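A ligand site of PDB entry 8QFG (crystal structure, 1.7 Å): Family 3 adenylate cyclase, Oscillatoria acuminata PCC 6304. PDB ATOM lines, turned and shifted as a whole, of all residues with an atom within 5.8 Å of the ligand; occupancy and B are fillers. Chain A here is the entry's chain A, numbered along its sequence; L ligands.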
ATOM      1  N   TYR A   6      20.640   2.718   0.263  1.00  0.00           N
ATOM      2  CA  TYR A   6      19.986   2.096   1.402  1.00  0.00           C
ATOM      3  C   TYR A   6      20.871   0.988   1.937  1.00  0.00           C
ATOM      4  O   TYR A   6      21.811   0.530   1.282  1.00  0.00           O
ATOM      5  CB  TYR A   6      18.604   1.529   1.038  1.00  0.00           C
ATOM      6  CG  TYR A   6      18.658   0.178   0.335  1.00  0.00           C
ATOM      7  CD1 TYR A   6      18.750  -0.998   1.067  1.00  0.00           C
ATOM      8  CD2 TYR A   6      18.578   0.082  -1.042  1.00  0.00           C
ATOM      9  CE1 TYR A   6      18.791  -2.247   0.438  1.00  0.00           C
ATOM     10  CE2 TYR A   6      18.618  -1.138  -1.683  1.00  0.00           C
ATOM     11  CZ  TYR A   6      18.732  -2.297  -0.939  1.00  0.00           C
ATOM     12  OH  TYR A   6      18.812  -3.485  -1.571  1.00  0.00           O
ATOM     13  N   SER A   8      20.556  -2.617   4.539  1.00  0.00           N
ATOM     14  CA  SER A   8      19.625  -3.606   5.042  1.00  0.00           C
ATOM     15  C   SER A   8      20.395  -4.691   5.778  1.00  0.00           C
ATOM     16  O   SER A   8      21.621  -4.803   5.657  1.00  0.00           O
ATOM     17  CB  SER A   8      18.798  -4.217   3.895  1.00  0.00           C
ATOM     18  OG  SER A   8      19.590  -5.147   3.185  1.00  0.00           O
ATOM     19  N   LEU A  14      22.764 -16.168   4.581  1.00  0.00           N
ATOM     20  CA  LEU A  14      22.715 -16.275   3.123  1.00  0.00           C
ATOM     21  C   LEU A  14      24.042 -16.841   2.641  1.00  0.00           C
ATOM     22  O   LEU A  14      25.107 -16.293   2.924  1.00  0.00           O
ATOM     23  CB  LEU A  14      22.452 -14.910   2.494  1.00  0.00           C
ATOM     24  CG  LEU A  14      21.152 -14.216   2.931  1.00  0.00           C
ATOM     25  CD1 LEU A  14      20.970 -12.891   2.180  1.00  0.00           C
ATOM     26  CD2 LEU A  14      19.944 -15.134   2.729  1.00  0.00           C
ATOM     27  N   ILE A  22      21.210 -13.290  -6.002  1.00  0.00           N
ATOM     28  CA  ILE A  22      20.792 -11.901  -5.872  1.00  0.00           C
ATOM     29  C   ILE A  22      21.378 -11.067  -7.008  1.00  0.00           C
ATOM     30  O   ILE A  22      20.650 -10.451  -7.790  1.00  0.00           O
ATOM     31  CB  ILE A  22      21.231 -11.323  -4.517  1.00  0.00           C
ATOM     32  CG1 ILE A  22      20.456 -11.947  -3.364  1.00  0.00           C
ATOM     33  CG2 ILE A  22      21.039  -9.776  -4.514  1.00  0.00           C
ATOM     34  CD1 ILE A  22      18.978 -11.847  -3.481  1.00  0.00           C
ATOM     35  N   ILE A  25      19.901 -11.873 -10.757  1.00  0.00           N
ATOM     36  CA  ILE A  25      18.569 -11.365 -11.027  1.00  0.00           C
ATOM     37  C   ILE A  25      18.587  -9.834 -11.048  1.00  0.00           C
ATOM     38  O   ILE A  25      17.980  -9.209 -11.921  1.00  0.00           O
ATOM     39  CB  ILE A  25      17.558 -11.898  -9.996  1.00  0.00           C
ATOM     40  CG1 ILE A  25      17.618 -13.435  -9.912  1.00  0.00           C
ATOM     41  CG2 ILE A  25      16.119 -11.499 -10.367  1.00  0.00           C
ATOM     42  CD1 ILE A  25      17.008 -14.006  -8.637  1.00  0.00           C
ATOM     43  N   SER A  26      19.283  -9.211 -10.090  1.00  0.00           N
ATOM     44  CA  SER A  26      19.360  -7.755 -10.064  1.00  0.00           C
ATOM     45  C   SER A  26      19.981  -7.211 -11.346  1.00  0.00           C
ATOM     46  O   SER A  26      19.522  -6.215 -11.902  1.00  0.00           O
ATOM     47  CB  SER A  26      20.152  -7.274  -8.835  1.00  0.00           C
ATOM     48  OG  SER A  26      19.563  -7.755  -7.637  1.00  0.00           O
ATOM     49  N   LYS A  29      17.414  -7.591 -14.366  1.00  0.00           N
ATOM     50  CA  LYS A  29      16.316  -6.634 -14.373  1.00  0.00           C
ATOM     51  C   LYS A  29      16.833  -5.200 -14.479  1.00  0.00           C
ATOM     52  O   LYS A  29      16.286  -4.388 -15.229  1.00  0.00           O
ATOM     53  CB  LYS A  29      15.460  -6.815 -13.124  1.00  0.00           C
ATOM     54  CG  LYS A  29      15.005  -8.257 -12.882  1.00  0.00           C
ATOM     55  CD  LYS A  29      13.628  -8.343 -12.252  1.00  0.00           C
ATOM     56  CE  LYS A  29      12.550  -7.820 -13.217  1.00  0.00           C
ATOM     57  NZ  LYS A  29      11.266  -8.583 -13.109  1.00  0.00           N
ATOM     58  N   ASN A  30      17.884  -4.842 -13.734  1.00  0.00           N
ATOM     59  CA  ASN A  30      18.381  -3.474 -13.817  1.00  0.00           C
ATOM     60  C   ASN A  30      18.840  -3.136 -15.239  1.00  0.00           C
ATOM     61  O   ASN A  30      18.604  -2.022 -15.732  1.00  0.00           O
ATOM     62  CB  ASN A  30      19.534  -3.276 -12.830  1.00  0.00           C
ATOM     63  CG  ASN A  30      19.074  -3.282 -11.393  1.00  0.00           C
ATOM     64  OD1 ASN A  30      17.860  -3.233 -11.102  1.00  0.00           O
ATOM     65  ND2 ASN A  30      20.038  -3.332 -10.452  1.00  0.00           N
ATOM     66  N   VAL A  35      18.970   0.859 -15.259  1.00  0.00           N
ATOM     67  CA  VAL A  35      19.287   1.211 -13.879  1.00  0.00           C
ATOM     68  C   VAL A  35      20.721   0.761 -13.593  1.00  0.00           C
ATOM     69  O   VAL A  35      21.060  -0.411 -13.777  1.00  0.00           O
ATOM     70  CB  VAL A  35      18.295   0.578 -12.888  1.00  0.00           C
ATOM     71  CG1 VAL A  35      18.838   0.615 -11.475  1.00  0.00           C
ATOM     72  CG2 VAL A  35      16.936   1.294 -12.970  1.00  0.00           C
ATOM     73  N   LEU A  39      25.767  -3.117  -5.611  1.00  0.00           N
ATOM     74  CA  LEU A  39      25.239  -3.777  -4.421  1.00  0.00           C
ATOM     75  C   LEU A  39      26.427  -4.381  -3.665  1.00  0.00           C
ATOM     76  O   LEU A  39      27.031  -5.369  -4.095  1.00  0.00           O
ATOM     77  CB  LEU A  39      24.230  -4.851  -4.815  1.00  0.00           C
ATOM     78  CG  LEU A  39      23.803  -5.851  -3.745  1.00  0.00           C
ATOM     79  CD1 LEU A  39      23.302  -5.147  -2.495  1.00  0.00           C
ATOM     80  CD2 LEU A  39      22.715  -6.809  -4.295  1.00  0.00           C
ATOM     81  N   PHE A  46      23.629  -5.658   3.730  1.00  0.00           N
ATOM     82  CA  PHE A  46      23.643  -5.200   2.349  1.00  0.00           C
ATOM     83  C   PHE A  46      23.689  -3.684   2.348  1.00  0.00           C
ATOM     84  O   PHE A  46      23.047  -3.028   3.162  1.00  0.00           O
ATOM     85  CB  PHE A  46      22.405  -5.678   1.576  1.00  0.00           C
ATOM     86  CG  PHE A  46      22.336  -7.159   1.322  1.00  0.00           C
ATOM     87  CD1 PHE A  46      23.236  -7.768   0.445  1.00  0.00           C
ATOM     88  CD2 PHE A  46      21.346  -7.946   1.915  1.00  0.00           C
ATOM     89  CE1 PHE A  46      23.160  -9.152   0.170  1.00  0.00           C
ATOM     90  CE2 PHE A  46      21.266  -9.334   1.653  1.00  0.00           C
ATOM     91  CZ  PHE A  46      22.171  -9.929   0.774  1.00  0.00           C
ATOM     92  N   GLN A  48      23.297  -0.734  -0.974  1.00  0.00           N
ATOM     93  CA  GLN A  48      23.138  -0.620  -2.416  1.00  0.00           C
ATOM     94  C   GLN A  48      22.791   0.788  -2.897  1.00  0.00           C
ATOM     95  O   GLN A  48      21.972   1.434  -2.264  1.00  0.00           O
ATOM     96  CB  GLN A  48      21.962  -1.515  -2.948  1.00  0.00           C
ATOM     97  CG  GLN A  48      21.485  -1.154  -4.353  1.00  0.00           C
ATOM     98  CD  GLN A  48      20.799  -2.242  -5.129  1.00  0.00           C
ATOM     99  OE1 GLN A  48      20.488  -2.080  -6.302  1.00  0.00           O
ATOM    100  NE2 GLN A  48      20.550  -3.371  -4.501  1.00  0.00           N
ATOM    101  N   LEU A  50      21.330   2.693  -6.305  1.00  0.00           N
ATOM    102  CA  LEU A  50      20.688   2.448  -7.593  1.00  0.00           C
ATOM    103  C   LEU A  50      20.112   3.746  -8.159  1.00  0.00           C
ATOM    104  O   LEU A  50      19.511   4.538  -7.423  1.00  0.00           O
ATOM    105  CB  LEU A  50      19.581   1.381  -7.501  1.00  0.00           C
ATOM    106  CG  LEU A  50      18.356   1.584  -6.617  1.00  0.00           C
ATOM    107  CD1 LEU A  50      17.313   0.483  -6.945  1.00  0.00           C
ATOM    108  CD2 LEU A  50      18.703   1.506  -5.155  1.00  0.00           C
ATOM    109  N   ILE A  60      11.642  -0.812  -8.710  1.00  0.00           N
ATOM    110  CA  ILE A  60      12.670  -1.736  -8.247  1.00  0.00           C
ATOM    111  C   ILE A  60      12.791  -1.694  -6.734  1.00  0.00           C
ATOM    112  O   ILE A  60      12.681  -2.721  -6.045  1.00  0.00           O
ATOM    113  CB  ILE A  60      14.020  -1.435  -8.922  1.00  0.00           C
ATOM    114  CG1 ILE A  60      13.915  -1.678 -10.435  1.00  0.00           C
ATOM    115  CG2 ILE A  60      15.150  -2.288  -8.304  1.00  0.00           C
ATOM    116  CD1 ILE A  60      14.847  -0.817 -11.233  1.00  0.00           C
ATOM    117  N   ARG A  63      10.147  -3.769  -5.128  1.00  0.00           N
ATOM    118  CA  ARG A  63      10.421  -5.197  -5.161  1.00  0.00           C
ATOM    119  C   ARG A  63      11.471  -5.567  -4.116  1.00  0.00           C
ATOM    120  O   ARG A  63      11.393  -6.626  -3.484  1.00  0.00           O
ATOM    121  CB  ARG A  63      10.900  -5.599  -6.550  1.00  0.00           C
ATOM    122  CG  ARG A  63       9.833  -6.166  -7.482  1.00  0.00           C
ATOM    123  CD  ARG A  63       9.749  -5.301  -8.741  1.00  0.00           C
ATOM    124  NE  ARG A  63      10.987  -5.355  -9.516  1.00  0.00           N
ATOM    125  CZ  ARG A  63      11.130  -4.850 -10.734  1.00  0.00           C
ATOM    126  NH1 ARG A  63      10.121  -4.265 -11.367  1.00  0.00           N
ATOM    127  NH2 ARG A  63      12.329  -4.909 -11.327  1.00  0.00           N
ATOM    128  N   ILE A  64      12.476  -4.715  -3.935  1.00  0.00           N
ATOM    129  CA  ILE A  64      13.504  -4.961  -2.920  1.00  0.00           C
ATOM    130  C   ILE A  64      12.900  -4.906  -1.531  1.00  0.00           C
ATOM    131  O   ILE A  64      13.240  -5.710  -0.664  1.00  0.00           O
ATOM    132  CB  ILE A  64      14.649  -3.937  -3.086  1.00  0.00           C
ATOM    133  CG1 ILE A  64      15.426  -4.191  -4.368  1.00  0.00           C
ATOM    134  CG2 ILE A  64      15.582  -3.949  -1.872  1.00  0.00           C
ATOM    135  CD1 ILE A  64      15.914  -2.947  -5.047  1.00  0.00           C
ATOM    136  N   LEU A  65      12.009  -3.937  -1.298  1.00  0.00           N
ATOM    137  CA  LEU A  65      11.366  -3.824   0.013  1.00  0.00           C
ATOM    138  C   LEU A  65      10.607  -5.106   0.360  1.00  0.00           C
ATOM    139  O   LEU A  65      10.679  -5.588   1.499  1.00  0.00           O
ATOM    140  CB  LEU A  65      10.415  -2.632   0.019  1.00  0.00           C
ATOM    141  CG  LEU A  65      11.004  -1.287   0.472  1.00  0.00           C
ATOM    142  CD1 LEU A  65       9.977  -0.173   0.335  1.00  0.00           C
ATOM    143  CD2 LEU A  65      11.552  -1.332   1.911  1.00  0.00           C
ATOM    144  N   ASP A  67      11.304  -8.093  -0.659  1.00  0.00           N
ATOM    145  CA  ASP A  67      12.175  -9.258  -0.593  1.00  0.00           C
ATOM    146  C   ASP A  67      12.365  -9.689   0.858  1.00  0.00           C
ATOM    147  O   ASP A  67      12.753  -8.880   1.714  1.00  0.00           O
ATOM    148  CB  ASP A  67      13.510  -8.935  -1.248  1.00  0.00           C
ATOM    149  CG  ASP A  67      14.235 -10.166  -1.747  1.00  0.00           C
ATOM    150  OD1 ASP A  67      14.497 -11.060  -0.916  1.00  0.00           O
ATOM    151  OD2 ASP A  67      14.551 -10.231  -2.958  1.00  0.00           O
ATOM    152  N   ARG A  69      14.527 -11.827   1.953  1.00  0.00           N
ATOM    153  CA  ARG A  69      15.899 -12.218   2.242  1.00  0.00           C
ATOM    154  C   ARG A  69      16.669 -11.164   3.040  1.00  0.00           C
ATOM    155  O   ARG A  69      17.814 -11.435   3.450  1.00  0.00           O
ATOM    156  CB  ARG A  69      16.640 -12.537   0.940  1.00  0.00           C
ATOM    157  CG  ARG A  69      15.949 -13.593   0.087  1.00  0.00           C
ATOM    158  CD  ARG A  69      16.671 -13.832  -1.238  1.00  0.00           C
ATOM    159  NE  ARG A  69      16.081 -13.061  -2.319  1.00  0.00           N
ATOM    160  CZ  ARG A  69      16.330 -13.268  -3.607  1.00  0.00           C
ATOM    161  NH1 ARG A  69      17.127 -14.253  -4.011  1.00  0.00           N
ATOM    162  NH2 ARG A  69      15.780 -12.463  -4.503  1.00  0.00           N
ATOM    163  N   HIS A  70      16.086 -10.000   3.283  1.00  0.00           N
ATOM    164  CA  HIS A  70      16.709  -9.002   4.138  1.00  0.00           C
ATOM    165  C   HIS A  70      15.611  -8.229   4.854  1.00  0.00           C
ATOM    166  O   HIS A  70      14.437  -8.312   4.482  1.00  0.00           O
ATOM    167  CB  HIS A  70      17.626  -8.061   3.334  1.00  0.00           C
ATOM    168  CG  HIS A  70      16.918  -7.228   2.317  1.00  0.00           C
ATOM    169  ND1 HIS A  70      17.564  -6.263   1.576  1.00  0.00           N
ATOM    170  CD2 HIS A  70      15.625  -7.239   1.886  1.00  0.00           C
ATOM    171  CE1 HIS A  70      16.699  -5.702   0.743  1.00  0.00           C
ATOM    172  NE2 HIS A  70      15.524  -6.279   0.919  1.00  0.00           N
ATOM    173  N   TRP A  90      25.856  -1.637 -13.705  1.00  0.00           N
ATOM    174  CA  TRP A  90      25.474  -2.156 -12.405  1.00  0.00           C
ATOM    175  C   TRP A  90      26.199  -3.480 -12.179  1.00  0.00           C
ATOM    176  O   TRP A  90      26.279  -4.314 -13.096  1.00  0.00           O
ATOM    177  CB  TRP A  90      23.955  -2.374 -12.309  1.00  0.00           C
ATOM    178  CG  TRP A  90      23.480  -2.711 -10.931  1.00  0.00           C
ATOM    179  CD1 TRP A  90      22.924  -1.843 -10.024  1.00  0.00           C
ATOM    180  CD2 TRP A  90      23.533  -3.987 -10.283  1.00  0.00           C
ATOM    181  NE1 TRP A  90      22.611  -2.504  -8.859  1.00  0.00           N
ATOM    182  CE2 TRP A  90      22.979  -3.824  -8.995  1.00  0.00           C
ATOM    183  CE3 TRP A  90      23.993  -5.258 -10.671  1.00  0.00           C
ATOM    184  CZ2 TRP A  90      22.862  -4.888  -8.092  1.00  0.00           C
ATOM    185  CZ3 TRP A  90      23.881  -6.309  -9.770  1.00  0.00           C
ATOM    186  CH2 TRP A  90      23.319  -6.123  -8.499  1.00  0.00           C
HETATM  187  N1  LIG L   1      15.937  -6.918  -7.938  1.00  0.00           N
HETATM  188  C1  LIG L   1      15.960  -5.961  -9.031  1.00  0.00           C
HETATM  189  O1  LIG L   1      15.287  -6.130  -9.959  1.00  0.00           O
HETATM  190  N2  LIG L   1      16.852  -4.813  -8.972  1.00  0.00           N
HETATM  191  C2  LIG L   1      17.671  -4.647  -7.799  1.00  0.00           C
HETATM  192  O2  LIG L   1      18.355  -3.729  -7.754  1.00  0.00           O
HETATM  193  C3  LIG L   1      17.645  -5.621  -6.658  1.00  0.00           C
HETATM  194  N3  LIG L   1      18.473  -5.437  -5.499  1.00  0.00           N
HETATM  195  C4  LIG L   1      18.409  -6.439  -4.397  1.00  0.00           C
HETATM  196  C5  LIG L   1      19.222  -6.254  -3.282  1.00  0.00           C
HETATM  197  C6  LIG L   1      19.177  -7.170  -2.228  1.00  0.00           C
HETATM  198  C7  LIG L   1      20.172  -6.694  -1.180  1.00  0.00           C
HETATM  199  C8  LIG L   1      18.330  -8.268  -2.308  1.00  0.00           C
HETATM  200  C9  LIG L   1      18.338  -9.236  -1.138  1.00  0.00           C
HETATM  201  C10 LIG L   1      17.532  -8.442  -3.414  1.00  0.00           C
HETATM  202  C11 LIG L   1      17.549  -7.540  -4.475  1.00  0.00           C
HETATM  203  N4  LIG L   1      16.687  -7.710  -5.687  1.00  0.00           N
HETATM  204  C12 LIG L   1      16.773  -6.749  -6.750  1.00  0.00           C
HETATM  205  C13 LIG L   1      15.770  -8.819  -5.890  1.00  0.00           C
HETATM  206  C14 LIG L   1      14.305  -8.350  -5.879  1.00  0.00           C
HETATM  207  O3  LIG L   1      13.887  -8.158  -4.574  1.00  0.00           O
HETATM  208  C15 LIG L   1      13.422  -9.391  -6.559  1.00  0.00           C
HETATM  209  O4  LIG L   1      13.721 -10.655  -6.071  1.00  0.00           O
HETATM  210  C16 LIG L   1      13.608  -9.368  -8.080  1.00  0.00           C
HETATM  211  O5  LIG L   1      12.975  -8.250  -8.624  1.00  0.00           O
HETATM  212  C17 LIG L   1      12.996 -10.635  -8.662  1.00  0.00           C
HETATM  213  O6  LIG L   1      12.833 -10.459 -10.019  1.00  0.00           O
HETATM  214  P1  LIG L   1      11.838 -11.481 -10.816  1.00  0.00           P
HETATM  215  O7  LIG L   1      10.450 -10.923 -10.769  1.00  0.00           O
HETATM  216  O8  LIG L   1      11.864 -12.828 -10.149  1.00  0.00           O
HETATM  217  O9  LIG L   1      12.298 -11.617 -12.236  1.00  0.00           O
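OH of Tyr 6 touches C5 of the ligand, 3.3 Å away.
Ile 22 touches the ligand.
Ile 25 touches the ligand (CG2 to O6, 3.5 Å).
Leu 39 touches the ligand.
Phe 46 touches the ligand (CG to C7, 3.3 Å).
Ile 60 touches the ligand.
Ile 64 touches the ligand (CG1 to N3, 3.5 Å).
His 70 touches the ligand.
Hydrophobic or aromatic side chains that line the ligand: Ile 22, Ile 25, Leu 39, Phe 46, Ile 60 and Ile 64.
Of the 21 residues printed, 15 come within 4 Å of the ligand.
The nearest printed residue that does not touch the ligand is Leu 50 (4.4 Å).
A nitrogen (N3) of the ligand lies close to the side-chain hydroxyl of Ser 26.
The side-chain amide oxygen (OD1) of Asn 30 is in hydrogen-bond range of a nitrogen (N2) of the ligand (2.8 Å).
The guanidinium group (NH2) of Arg 69 is in hydrogen-bond range of an oxygen (O4) of the ligand (3.2 Å).
OD2 of Asp 67 lies within hydrogen-bond range of O3 of the ligand (2.7 Å).
The guanidinium group (NH2) of Arg 63 is in hydrogen-bond range of an oxygen (O1) of the ligand (3.5 Å).
The side-chain amide oxygen of Gln 48 sits close to an oxygen (O2) of the ligand (3.1 Å).
The backbone carbonyl oxygen (O) of Arg 63 is in hydrogen-bond range of an oxygen (O3) of the ligand, 3.1 Å away.
The side-chain amino group (NZ) of Lys 29 is in salt-bridge range of an oxygen (O9) of the ligand, at 3.3 Å.
The backbone carbonyl oxygen of Asn 30 lies within hydrogen-bond range of the backbone NH of Val 35.
O of Tyr 6 lies within hydrogen-bond range of N of Gln 48.
The backbone carbonyl oxygen (O) of Ile 22 sits at hydrogen-bond distance from the side-chain hydroxyl (OG) of Ser 26 (2.9 Å).
A ring nitrogen (ND1) of His 70 sits at hydrogen-bond distance from the side-chain hydroxyl (OG) of Ser 8, 2.8 Å away.
The indole nitrogen (NE1) of Trp 90 sits at hydrogen-bond distance from the side-chain amide oxygen (OE1) of Gln 48, at 3.4 Å.
The backbone carbonyl oxygen of Ile 64 lies within hydrogen-bond range of a ring nitrogen (NE2) of His 70.
The side-chain carboxylate (OD1) of Asp 67 is in salt-bridge range of the guanidinium group (NE) of Arg 69 (2.9 Å).
ND2 of Asn 30 sits close to NE1 of Trp 90 (3.1 Å).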
